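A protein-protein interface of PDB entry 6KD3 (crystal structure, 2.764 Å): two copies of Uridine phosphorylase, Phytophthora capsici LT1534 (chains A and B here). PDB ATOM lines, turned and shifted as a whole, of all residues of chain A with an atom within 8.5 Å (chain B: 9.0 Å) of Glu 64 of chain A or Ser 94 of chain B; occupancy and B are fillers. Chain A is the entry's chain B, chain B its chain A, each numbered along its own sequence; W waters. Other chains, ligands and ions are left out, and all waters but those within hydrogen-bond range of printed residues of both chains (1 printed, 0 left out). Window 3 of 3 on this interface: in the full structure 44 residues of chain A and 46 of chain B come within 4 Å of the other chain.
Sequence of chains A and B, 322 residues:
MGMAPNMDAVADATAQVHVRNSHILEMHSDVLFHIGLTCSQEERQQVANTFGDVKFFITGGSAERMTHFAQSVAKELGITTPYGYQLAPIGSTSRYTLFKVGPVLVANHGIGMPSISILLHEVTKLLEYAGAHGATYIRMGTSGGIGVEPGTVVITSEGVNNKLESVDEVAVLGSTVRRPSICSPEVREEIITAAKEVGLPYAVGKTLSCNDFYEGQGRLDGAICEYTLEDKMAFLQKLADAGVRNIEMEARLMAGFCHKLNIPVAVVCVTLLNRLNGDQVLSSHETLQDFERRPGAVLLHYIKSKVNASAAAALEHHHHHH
Glu 64 of chain A touches Ser 94 of chain B, and with the chains exchanged Ser 94 of chain A touches Glu 64 of chain B.
Arg 95 of chain A touches Gly 110 of chain B, and with the chains exchanged Gly 110 of chain A touches Arg 95 of chain B.
9 positions are printed for both chains.
Of the 4 pairs that touch across the chains among the printed residues, 4 have their exchanged pair printed and touching as well.
The backbone carbonyl oxygen (O) of Gly 61 of chain B lies within hydrogen-bond range of the backbone NH (N) of Gly 110 of chain B (3.4 Å).
N of Gly 110 of chain A sits at hydrogen-bond distance from O of Gly 61 of chain A, 2.9 Å away.
Glu 64 of chain A touches one residue of chain B.
Of the printed residues of chain B, Ser 94 of chain A touches Glu 64.
Of chain A, only Glu 64 (3.3 Å) comes within 4 Å of Ser 94 of chain B.
Printed residues of chain A within 4 Å of Gly 110 of chain B: Arg 95 (3.7 Å).
The nearest residue of chain B that does not touch Glu 64 of chain A is Ser 92 of chain B (5.3 Å).
The nearest residue of chain A that does not touch Ser 94 of chain B is Ser 62 of chain A (4.03 Å).
The nearest printed residue of chain B that does not touch Ser 94 of chain A is Ser 62 of chain B (4.4 Å).
Of the 16 printed residues of chain A, 4 touch a printed residue of chain B.
Ser 94 of chain B touches Glu 64 of chain A.
Ser 94 of chain A touches Glu 64 of chain B.
C of Gly 110 of chain B touches NE of Arg 95 of chain A, 3.7 Å away.
Gly 110 of chain A touches Arg 95 of chain B (C to NE, 3.1 Å).
Water W1 lies within hydrogen-bond range of N of Ser 62 of chain A and NH2 of Arg 95 of chain B.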
ATOM      1  N   GLY A  61      35.449  -1.495 -16.539  1.00  0.00           N
ATOM      2  CA  GLY A  61      34.093  -1.275 -16.087  1.00  0.00           C
ATOM      3  C   GLY A  61      33.193  -2.492 -16.184  1.00  0.00           C
ATOM      4  O   GLY A  61      32.811  -3.069 -15.159  1.00  0.00           O
ATOM      5  N   SER A  62      32.830  -2.884 -17.402  1.00  0.00           N
ATOM      6  CA  SER A  62      31.818  -3.915 -17.587  1.00  0.00           C
ATOM      7  C   SER A  62      32.412  -5.309 -17.431  1.00  0.00           C
ATOM      8  O   SER A  62      33.630  -5.493 -17.384  1.00  0.00           O
ATOM      9  CB  SER A  62      31.154  -3.766 -18.953  1.00  0.00           C
ATOM     10  OG  SER A  62      32.127  -3.606 -19.965  1.00  0.00           O
ATOM     11  N   ALA A  63      31.519  -6.294 -17.319  1.00  0.00           N
ATOM     12  CA  ALA A  63      31.894  -7.700 -17.238  1.00  0.00           C
ATOM     13  C   ALA A  63      32.121  -8.315 -18.606  1.00  0.00           C
ATOM     14  O   ALA A  63      32.956  -9.216 -18.755  1.00  0.00           O
ATOM     15  CB  ALA A  63      30.804  -8.490 -16.513  1.00  0.00           C
ATOM     16  N   GLU A  64      31.381  -7.842 -19.607  1.00  0.00           N
ATOM     17  CA  GLU A  64      31.507  -8.343 -20.965  1.00  0.00           C
ATOM     18  C   GLU A  64      32.734  -7.799 -21.681  1.00  0.00           C
ATOM     19  O   GLU A  64      33.072  -8.312 -22.750  1.00  0.00           O
ATOM     20  CB  GLU A  64      30.241  -8.012 -21.755  1.00  0.00           C
ATOM     21  CG  GLU A  64      30.164  -6.575 -22.217  1.00  0.00           C
ATOM     22  N   ARG A  65      33.404  -6.789 -21.123  1.00  0.00           N
ATOM     23  CA  ARG A  65      34.702  -6.348 -21.626  1.00  0.00           C
ATOM     24  C   ARG A  65      35.875  -7.007 -20.913  1.00  0.00           C
ATOM     25  O   ARG A  65      36.933  -7.213 -21.527  1.00  0.00           O
ATOM     26  CB  ARG A  65      34.845  -4.830 -21.503  1.00  0.00           C
ATOM     27  CG  ARG A  65      36.155  -4.307 -22.057  1.00  0.00           C
ATOM     28  CD  ARG A  65      36.391  -2.868 -21.636  1.00  0.00           C
ATOM     29  NE  ARG A  65      35.540  -1.979 -22.425  1.00  0.00           N
ATOM     30  CZ  ARG A  65      35.897  -0.762 -22.814  1.00  0.00           C
ATOM     31  NH1 ARG A  65      37.092  -0.278 -22.498  1.00  0.00           N
ATOM     32  NH2 ARG A  65      35.065  -0.029 -23.529  1.00  0.00           N
ATOM     33  N   MET A  66      35.716  -7.342 -19.630  1.00  0.00           N
ATOM     34  CA  MET A  66      36.784  -8.038 -18.930  1.00  0.00           C
ATOM     35  C   MET A  66      36.762  -9.532 -19.221  1.00  0.00           C
ATOM     36  O   MET A  66      37.822 -10.169 -19.258  1.00  0.00           O
ATOM     37  CB  MET A  66      36.676  -7.762 -17.435  1.00  0.00           C
ATOM     38  CG  MET A  66      36.594  -6.278 -17.119  1.00  0.00           C
ATOM     39  SD  MET A  66      38.227  -5.532 -17.103  1.00  0.00           S
ATOM     40  CE  MET A  66      38.336  -4.783 -18.721  1.00  0.00           C
ATOM     41  N   THR A  67      35.571 -10.101 -19.437  1.00  0.00           N
ATOM     42  CA  THR A  67      35.491 -11.482 -19.889  1.00  0.00           C
ATOM     43  C   THR A  67      36.069 -11.626 -21.278  1.00  0.00           C
ATOM     44  O   THR A  67      36.696 -12.646 -21.582  1.00  0.00           O
ATOM     45  CB  THR A  67      34.049 -11.969 -19.883  1.00  0.00           C
ATOM     46  OG1 THR A  67      33.381 -11.449 -18.728  1.00  0.00           O
ATOM     47  N   HIS A  68      35.876 -10.616 -22.130  1.00  0.00           N
ATOM     48  CA  HIS A  68      36.446 -10.667 -23.475  1.00  0.00           C
ATOM     49  C   HIS A  68      37.962 -10.688 -23.436  1.00  0.00           C
ATOM     50  O   HIS A  68      38.592 -11.308 -24.300  1.00  0.00           O
ATOM     51  CB  HIS A  68      35.970  -9.470 -24.303  1.00  0.00           C
ATOM     52  N   PHE A  69      38.551 -10.004 -22.448  1.00  0.00           N
ATOM     53  CA  PHE A  69      39.999  -9.924 -22.269  1.00  0.00           C
ATOM     54  C   PHE A  69      40.545 -11.174 -21.595  1.00  0.00           C
ATOM     55  O   PHE A  69      41.632 -11.640 -21.939  1.00  0.00           O
ATOM     56  CB  PHE A  69      40.321  -8.679 -21.453  1.00  0.00           C
ATOM     57  CG  PHE A  69      41.753  -8.548 -21.029  1.00  0.00           C
ATOM     58  CD1 PHE A  69      42.646  -7.822 -21.782  1.00  0.00           C
ATOM     59  CD2 PHE A  69      42.181  -9.068 -19.825  1.00  0.00           C
ATOM     60  CE1 PHE A  69      43.951  -7.648 -21.372  1.00  0.00           C
ATOM     61  CE2 PHE A  69      43.498  -8.910 -19.417  1.00  0.00           C
ATOM     62  CZ  PHE A  69      44.381  -8.195 -20.202  1.00  0.00           C
ATOM     63  N   ALA A  70      39.795 -11.733 -20.643  1.00  0.00           N
ATOM     64  CA  ALA A  70      40.278 -12.887 -19.891  1.00  0.00           C
ATOM     65  C   ALA A  70      40.266 -14.152 -20.748  1.00  0.00           C
ATOM     66  O   ALA A  70      41.205 -14.955 -20.683  1.00  0.00           O
ATOM     67  CB  ALA A  70      39.452 -13.059 -18.612  1.00  0.00           C
ATOM     68  N   GLN A  71      39.220 -14.348 -21.558  1.00  0.00           N
ATOM     69  CA  GLN A  71      39.263 -15.343 -22.618  1.00  0.00           C
ATOM     70  C   GLN A  71      40.183 -14.940 -23.769  1.00  0.00           C
ATOM     71  O   GLN A  71      40.294 -15.697 -24.744  1.00  0.00           O
ATOM     72  CB  GLN A  71      37.857 -15.602 -23.155  1.00  0.00           C
ATOM     73  CG  GLN A  71      36.804 -15.690 -22.069  1.00  0.00           C
ATOM     74  N   SER A  94      26.722  -9.154  -8.189  1.00  0.00           N
ATOM     75  CA  SER A  94      26.896  -9.389  -9.611  1.00  0.00           C
ATOM     76  C   SER A  94      27.659  -8.258 -10.273  1.00  0.00           C
ATOM     77  O   SER A  94      28.221  -8.451 -11.360  1.00  0.00           O
ATOM     78  CB  SER A  94      25.534  -9.576 -10.272  1.00  0.00           C
ATOM     79  OG  SER A  94      24.675 -10.314  -9.419  1.00  0.00           O
ATOM     80  N   ARG A  95      27.674  -7.092  -9.625  1.00  0.00           N
ATOM     81  CA  ARG A  95      28.432  -5.938 -10.085  1.00  0.00           C
ATOM     82  C   ARG A  95      29.823  -6.337 -10.542  1.00  0.00           C
ATOM     83  O   ARG A  95      30.173  -6.208 -11.721  1.00  0.00           O
ATOM     84  CB  ARG A  95      28.523  -4.930  -8.950  1.00  0.00           C
ATOM     85  CG  ARG A  95      28.689  -3.532  -9.400  1.00  0.00           C
ATOM     86  CD  ARG A  95      29.074  -2.692  -8.236  1.00  0.00           C
ATOM     87  NE  ARG A  95      28.084  -2.697  -7.149  1.00  0.00           N
ATOM     88  CZ  ARG A  95      28.237  -3.331  -5.988  1.00  0.00           C
ATOM     89  NH1 ARG A  95      29.329  -4.050  -5.755  1.00  0.00           N
ATOM     90  NH2 ARG A  95      27.285  -3.263  -5.064  1.00  0.00           N
ATOM     91  N   THR A  97      32.906  -8.947 -11.368  1.00  0.00           N
ATOM     92  CA  THR A  97      33.070 -10.271 -11.956  1.00  0.00           C
ATOM     93  C   THR A  97      34.531 -10.445 -12.344  1.00  0.00           C
ATOM     94  O   THR A  97      35.115  -9.557 -12.973  1.00  0.00           O
ATOM     95  CB  THR A  97      32.161 -10.466 -13.179  1.00  0.00           C
ATOM     96  N   ASN A 108      36.303  -6.982 -13.389  1.00  0.00           N
ATOM     97  CA  ASN A 108      35.569  -5.753 -13.665  1.00  0.00           C
ATOM     98  C   ASN A 108      35.338  -4.970 -12.377  1.00  0.00           C
ATOM     99  O   ASN A 108      35.172  -5.544 -11.299  1.00  0.00           O
ATOM    100  CB  ASN A 108      34.224  -6.058 -14.332  1.00  0.00           C
ATOM    101  CG  ASN A 108      33.108  -6.299 -13.328  1.00  0.00           C
ATOM    102  N   GLY A 110      33.265  -1.740 -12.616  1.00  0.00           N
ATOM    103  CA  GLY A 110      32.107  -0.882 -12.765  1.00  0.00           C
ATOM    104  C   GLY A 110      32.491   0.584 -12.917  1.00  0.00           C
ATOM    105  O   GLY A 110      33.475   0.894 -13.593  1.00  0.00           O
ATOM    106  N   PHE B  33      24.668   7.142 -23.748  1.00  0.00           N
ATOM    107  CA  PHE B  33      25.629   6.077 -24.002  1.00  0.00           C
ATOM    108  C   PHE B  33      25.340   4.875 -23.128  1.00  0.00           C
ATOM    109  O   PHE B  33      25.170   3.759 -23.628  1.00  0.00           O
ATOM    110  CB  PHE B  33      27.068   6.557 -23.780  1.00  0.00           C
ATOM    111  CG  PHE B  33      27.699   7.183 -24.997  1.00  0.00           C
ATOM    112  N   HIS B  34      25.207   5.105 -21.821  1.00  0.00           N
ATOM    113  CA  HIS B  34      25.484   4.053 -20.844  1.00  0.00           C
ATOM    114  C   HIS B  34      24.388   3.008 -20.745  1.00  0.00           C
ATOM    115  O   HIS B  34      24.674   1.892 -20.315  1.00  0.00           O
ATOM    116  CB  HIS B  34      25.738   4.681 -19.478  1.00  0.00           C
ATOM    117  CG  HIS B  34      26.896   5.629 -19.472  1.00  0.00           C
ATOM    118  ND1 HIS B  34      26.813   6.905 -19.989  1.00  0.00           N
ATOM    119  CD2 HIS B  34      28.170   5.483 -19.028  1.00  0.00           C
ATOM    120  CE1 HIS B  34      27.983   7.505 -19.856  1.00  0.00           C
ATOM    121  NE2 HIS B  34      28.822   6.667 -19.272  1.00  0.00           N
ATOM    122  N   ILE B  35      23.157   3.347 -21.123  1.00  0.00           N
ATOM    123  CA  ILE B  35      22.052   2.400 -21.142  1.00  0.00           C
ATOM    124  C   ILE B  35      21.851   1.790 -22.529  1.00  0.00           C
ATOM    125  O   ILE B  35      21.273   0.695 -22.636  1.00  0.00           O
ATOM    126  CB  ILE B  35      20.758   3.092 -20.664  1.00  0.00           C
ATOM    127  CG1 ILE B  35      21.088   4.273 -19.739  1.00  0.00           C
ATOM    128  N   GLY B  36      22.331   2.447 -23.582  1.00  0.00           N
ATOM    129  CA  GLY B  36      22.127   1.998 -24.935  1.00  0.00           C
ATOM    130  C   GLY B  36      20.975   2.652 -25.669  1.00  0.00           C
ATOM    131  O   GLY B  36      20.356   1.996 -26.518  1.00  0.00           O
ATOM    132  N   GLY B  61      21.114  -1.549  -6.103  1.00  0.00           N
ATOM    133  CA  GLY B  61      22.497  -1.937  -6.313  1.00  0.00           C
ATOM    134  C   GLY B  61      22.761  -2.737  -7.577  1.00  0.00           C
ATOM    135  O   GLY B  61      23.327  -2.213  -8.539  1.00  0.00           O
ATOM    136  N   SER B  62      22.325  -3.996  -7.601  1.00  0.00           N
ATOM    137  CA  SER B  62      22.763  -4.956  -8.606  1.00  0.00           C
ATOM    138  C   SER B  62      21.573  -5.539  -9.360  1.00  0.00           C
ATOM    139  O   SER B  62      20.599  -5.991  -8.745  1.00  0.00           O
ATOM    140  CB  SER B  62      23.577  -6.071  -7.947  1.00  0.00           C
ATOM    141  OG  SER B  62      23.023  -6.432  -6.690  1.00  0.00           O
ATOM    142  N   ALA B  63      21.678  -5.571 -10.696  1.00  0.00           N
ATOM    143  CA  ALA B  63      20.702  -6.227 -11.566  1.00  0.00           C
ATOM    144  C   ALA B  63      20.420  -7.670 -11.158  1.00  0.00           C
ATOM    145  O   ALA B  63      19.620  -8.357 -11.806  1.00  0.00           O
ATOM    146  CB  ALA B  63      21.175  -6.204 -13.017  1.00  0.00           C
ATOM    147  N   GLU B  64      21.097  -8.149 -10.117  1.00  0.00           N
ATOM    148  CA  GLU B  64      20.628  -9.321  -9.396  1.00  0.00           C
ATOM    149  C   GLU B  64      19.446  -8.988  -8.493  1.00  0.00           C
ATOM    150  O   GLU B  64      18.664  -9.875  -8.148  1.00  0.00           O
ATOM    151  CB  GLU B  64      21.766  -9.926  -8.578  1.00  0.00           C
ATOM    152  CG  GLU B  64      21.591  -9.801  -7.107  1.00  0.00           C
ATOM    153  N   ILE B  90      17.707  -1.967 -21.289  1.00  0.00           N
ATOM    154  CA  ILE B  90      18.877  -1.130 -21.520  1.00  0.00           C
ATOM    155  C   ILE B  90      20.156  -1.953 -21.394  1.00  0.00           C
ATOM    156  O   ILE B  90      20.211  -2.939 -20.650  1.00  0.00           O
ATOM    157  CB  ILE B  90      18.895   0.077 -20.560  1.00  0.00           C
ATOM    158  CG1 ILE B  90      20.081  -0.052 -19.593  1.00  0.00           C
ATOM    159  N   GLY B  91      21.196  -1.528 -22.134  1.00  0.00           N
ATOM    160  CA  GLY B  91      22.455  -2.256 -22.192  1.00  0.00           C
ATOM    161  C   GLY B  91      23.707  -1.404 -22.356  1.00  0.00           C
ATOM    162  O   GLY B  91      24.025  -0.610 -21.464  1.00  0.00           O
ATOM    163  N   SER B  92      24.434  -1.576 -23.476  1.00  0.00           N
ATOM    164  CA  SER B  92      25.695  -0.881 -23.773  1.00  0.00           C
ATOM    165  C   SER B  92      26.766  -1.158 -22.712  1.00  0.00           C
ATOM    166  O   SER B  92      27.747  -1.866 -22.973  1.00  0.00           O
ATOM    167  CB  SER B  92      25.469   0.631 -23.915  1.00  0.00           C
ATOM    168  N   THR B  93      26.608  -0.580 -21.528  1.00  0.00           N
ATOM    169  CA  THR B  93      27.381  -1.003 -20.378  1.00  0.00           C
ATOM    170  C   THR B  93      26.583  -2.094 -19.684  1.00  0.00           C
ATOM    171  O   THR B  93      25.415  -1.880 -19.334  1.00  0.00           O
ATOM    172  CB  THR B  93      27.671   0.161 -19.420  1.00  0.00           C
ATOM    173  OG1 THR B  93      26.475   0.918 -19.192  1.00  0.00           O
ATOM    174  CG2 THR B  93      28.751   1.076 -19.996  1.00  0.00           C
ATOM    175  N   SER B  94      27.197  -3.270 -19.522  1.00  0.00           N
ATOM    176  CA  SER B  94      26.565  -4.316 -18.732  1.00  0.00           C
ATOM    177  C   SER B  94      26.410  -3.891 -17.278  1.00  0.00           C
ATOM    178  O   SER B  94      25.786  -4.617 -16.492  1.00  0.00           O
ATOM    179  CB  SER B  94      27.361  -5.619 -18.814  1.00  0.00           C
ATOM    180  OG  SER B  94      27.645  -6.004 -20.156  1.00  0.00           O
ATOM    181  N   ARG B  95      26.966  -2.725 -16.917  1.00  0.00           N
ATOM    182  CA  ARG B  95      26.788  -2.171 -15.576  1.00  0.00           C
ATOM    183  C   ARG B  95      25.342  -1.777 -15.337  1.00  0.00           C
ATOM    184  O   ARG B  95      24.777  -2.075 -14.282  1.00  0.00           O
ATOM    185  CB  ARG B  95      27.702  -0.960 -15.378  1.00  0.00           C
ATOM    186  CG  ARG B  95      28.186  -0.767 -13.967  1.00  0.00           C
ATOM    187  CD  ARG B  95      29.074   0.452 -13.865  1.00  0.00           C
ATOM    188  NE  ARG B  95      30.074   0.469 -14.929  1.00  0.00           N
ATOM    189  CZ  ARG B  95      30.146   1.406 -15.869  1.00  0.00           C
ATOM    190  NH1 ARG B  95      29.270   2.411 -15.859  1.00  0.00           N
ATOM    191  NH2 ARG B  95      31.091   1.335 -16.815  1.00  0.00           N
ATOM    192  N   TYR B  96      24.722  -1.134 -16.323  1.00  0.00           N
ATOM    193  CA  TYR B  96      23.332  -0.683 -16.250  1.00  0.00           C
ATOM    194  C   TYR B  96      22.419  -1.660 -16.994  1.00  0.00           C
ATOM    195  O   TYR B  96      22.456  -1.741 -18.230  1.00  0.00           O
ATOM    196  CB  TYR B  96      23.185   0.711 -16.845  1.00  0.00           C
ATOM    197  CG  TYR B  96      23.828   1.835 -16.062  1.00  0.00           C
ATOM    198  CD1 TYR B  96      23.759   1.884 -14.684  1.00  0.00           C
ATOM    199  CD2 TYR B  96      24.467   2.879 -16.721  1.00  0.00           C
ATOM    200  CE1 TYR B  96      24.325   2.938 -13.985  1.00  0.00           C
ATOM    201  CE2 TYR B  96      25.024   3.930 -16.031  1.00  0.00           C
ATOM    202  CZ  TYR B  96      24.957   3.949 -14.671  1.00  0.00           C
ATOM    203  OH  TYR B  96      25.513   4.998 -13.991  1.00  0.00           O
ATOM    204  N   THR B  97      21.586  -2.379 -16.238  1.00  0.00           N
ATOM    205  CA  THR B  97      20.521  -3.214 -16.773  1.00  0.00           C
ATOM    206  C   THR B  97      19.182  -2.626 -16.334  1.00  0.00           C
ATOM    207  O   THR B  97      19.055  -2.103 -15.218  1.00  0.00           O
ATOM    208  CB  THR B  97      20.656  -4.667 -16.302  1.00  0.00           C
ATOM    209  N   LEU B  98      18.196  -2.687 -17.218  1.00  0.00           N
ATOM    210  CA  LEU B  98      16.941  -1.987 -17.031  1.00  0.00           C
ATOM    211  C   LEU B  98      15.806  -2.951 -17.313  1.00  0.00           C
ATOM    212  O   LEU B  98      16.009  -4.019 -17.883  1.00  0.00           O
ATOM    213  CB  LEU B  98      16.853  -0.749 -17.951  1.00  0.00           C
ATOM    214  CG  LEU B  98      15.522  -0.195 -18.490  1.00  0.00           C
ATOM    215  N   ASN B 108      18.885  -0.847 -12.247  1.00  0.00           N
ATOM    216  CA  ASN B 108      20.084  -0.925 -11.409  1.00  0.00           C
ATOM    217  C   ASN B 108      21.051   0.216 -11.749  1.00  0.00           C
ATOM    218  O   ASN B 108      20.806   1.023 -12.641  1.00  0.00           O
ATOM    219  CB  ASN B 108      20.776  -2.279 -11.576  1.00  0.00           C
ATOM    220  CG  ASN B 108      21.134  -2.585 -13.017  1.00  0.00           C
ATOM    221  N   HIS B 109      22.160   0.304 -11.012  1.00  0.00           N
ATOM    222  CA  HIS B 109      22.974   1.516 -11.091  1.00  0.00           C
ATOM    223  C   HIS B 109      24.363   1.370 -10.495  1.00  0.00           C
ATOM    224  O   HIS B 109      24.949   2.388 -10.091  1.00  0.00           O
ATOM    225  CB  HIS B 109      22.259   2.709 -10.412  1.00  0.00           C
ATOM    226  CG  HIS B 109      22.298   2.691  -8.905  1.00  0.00           C
ATOM    227  ND1 HIS B 109      23.476   2.710  -8.177  1.00  0.00           N
ATOM    228  CD2 HIS B 109      21.297   2.708  -7.988  1.00  0.00           C
ATOM    229  CE1 HIS B 109      23.196   2.687  -6.885  1.00  0.00           C
ATOM    230  NE2 HIS B 109      21.882   2.683  -6.744  1.00  0.00           N
ATOM    231  N   GLY B 110      24.896   0.155 -10.398  1.00  0.00           N
ATOM    232  CA  GLY B 110      26.289  -0.001  -9.967  1.00  0.00           C
ATOM    233  C   GLY B 110      26.552   0.341  -8.503  1.00  0.00           C
ATOM    234  O   GLY B 110      25.714   0.124  -7.617  1.00  0.00           O
HETATM  235  O   HOH W   1      32.722  -0.783 -18.672  1.00  0.00           O
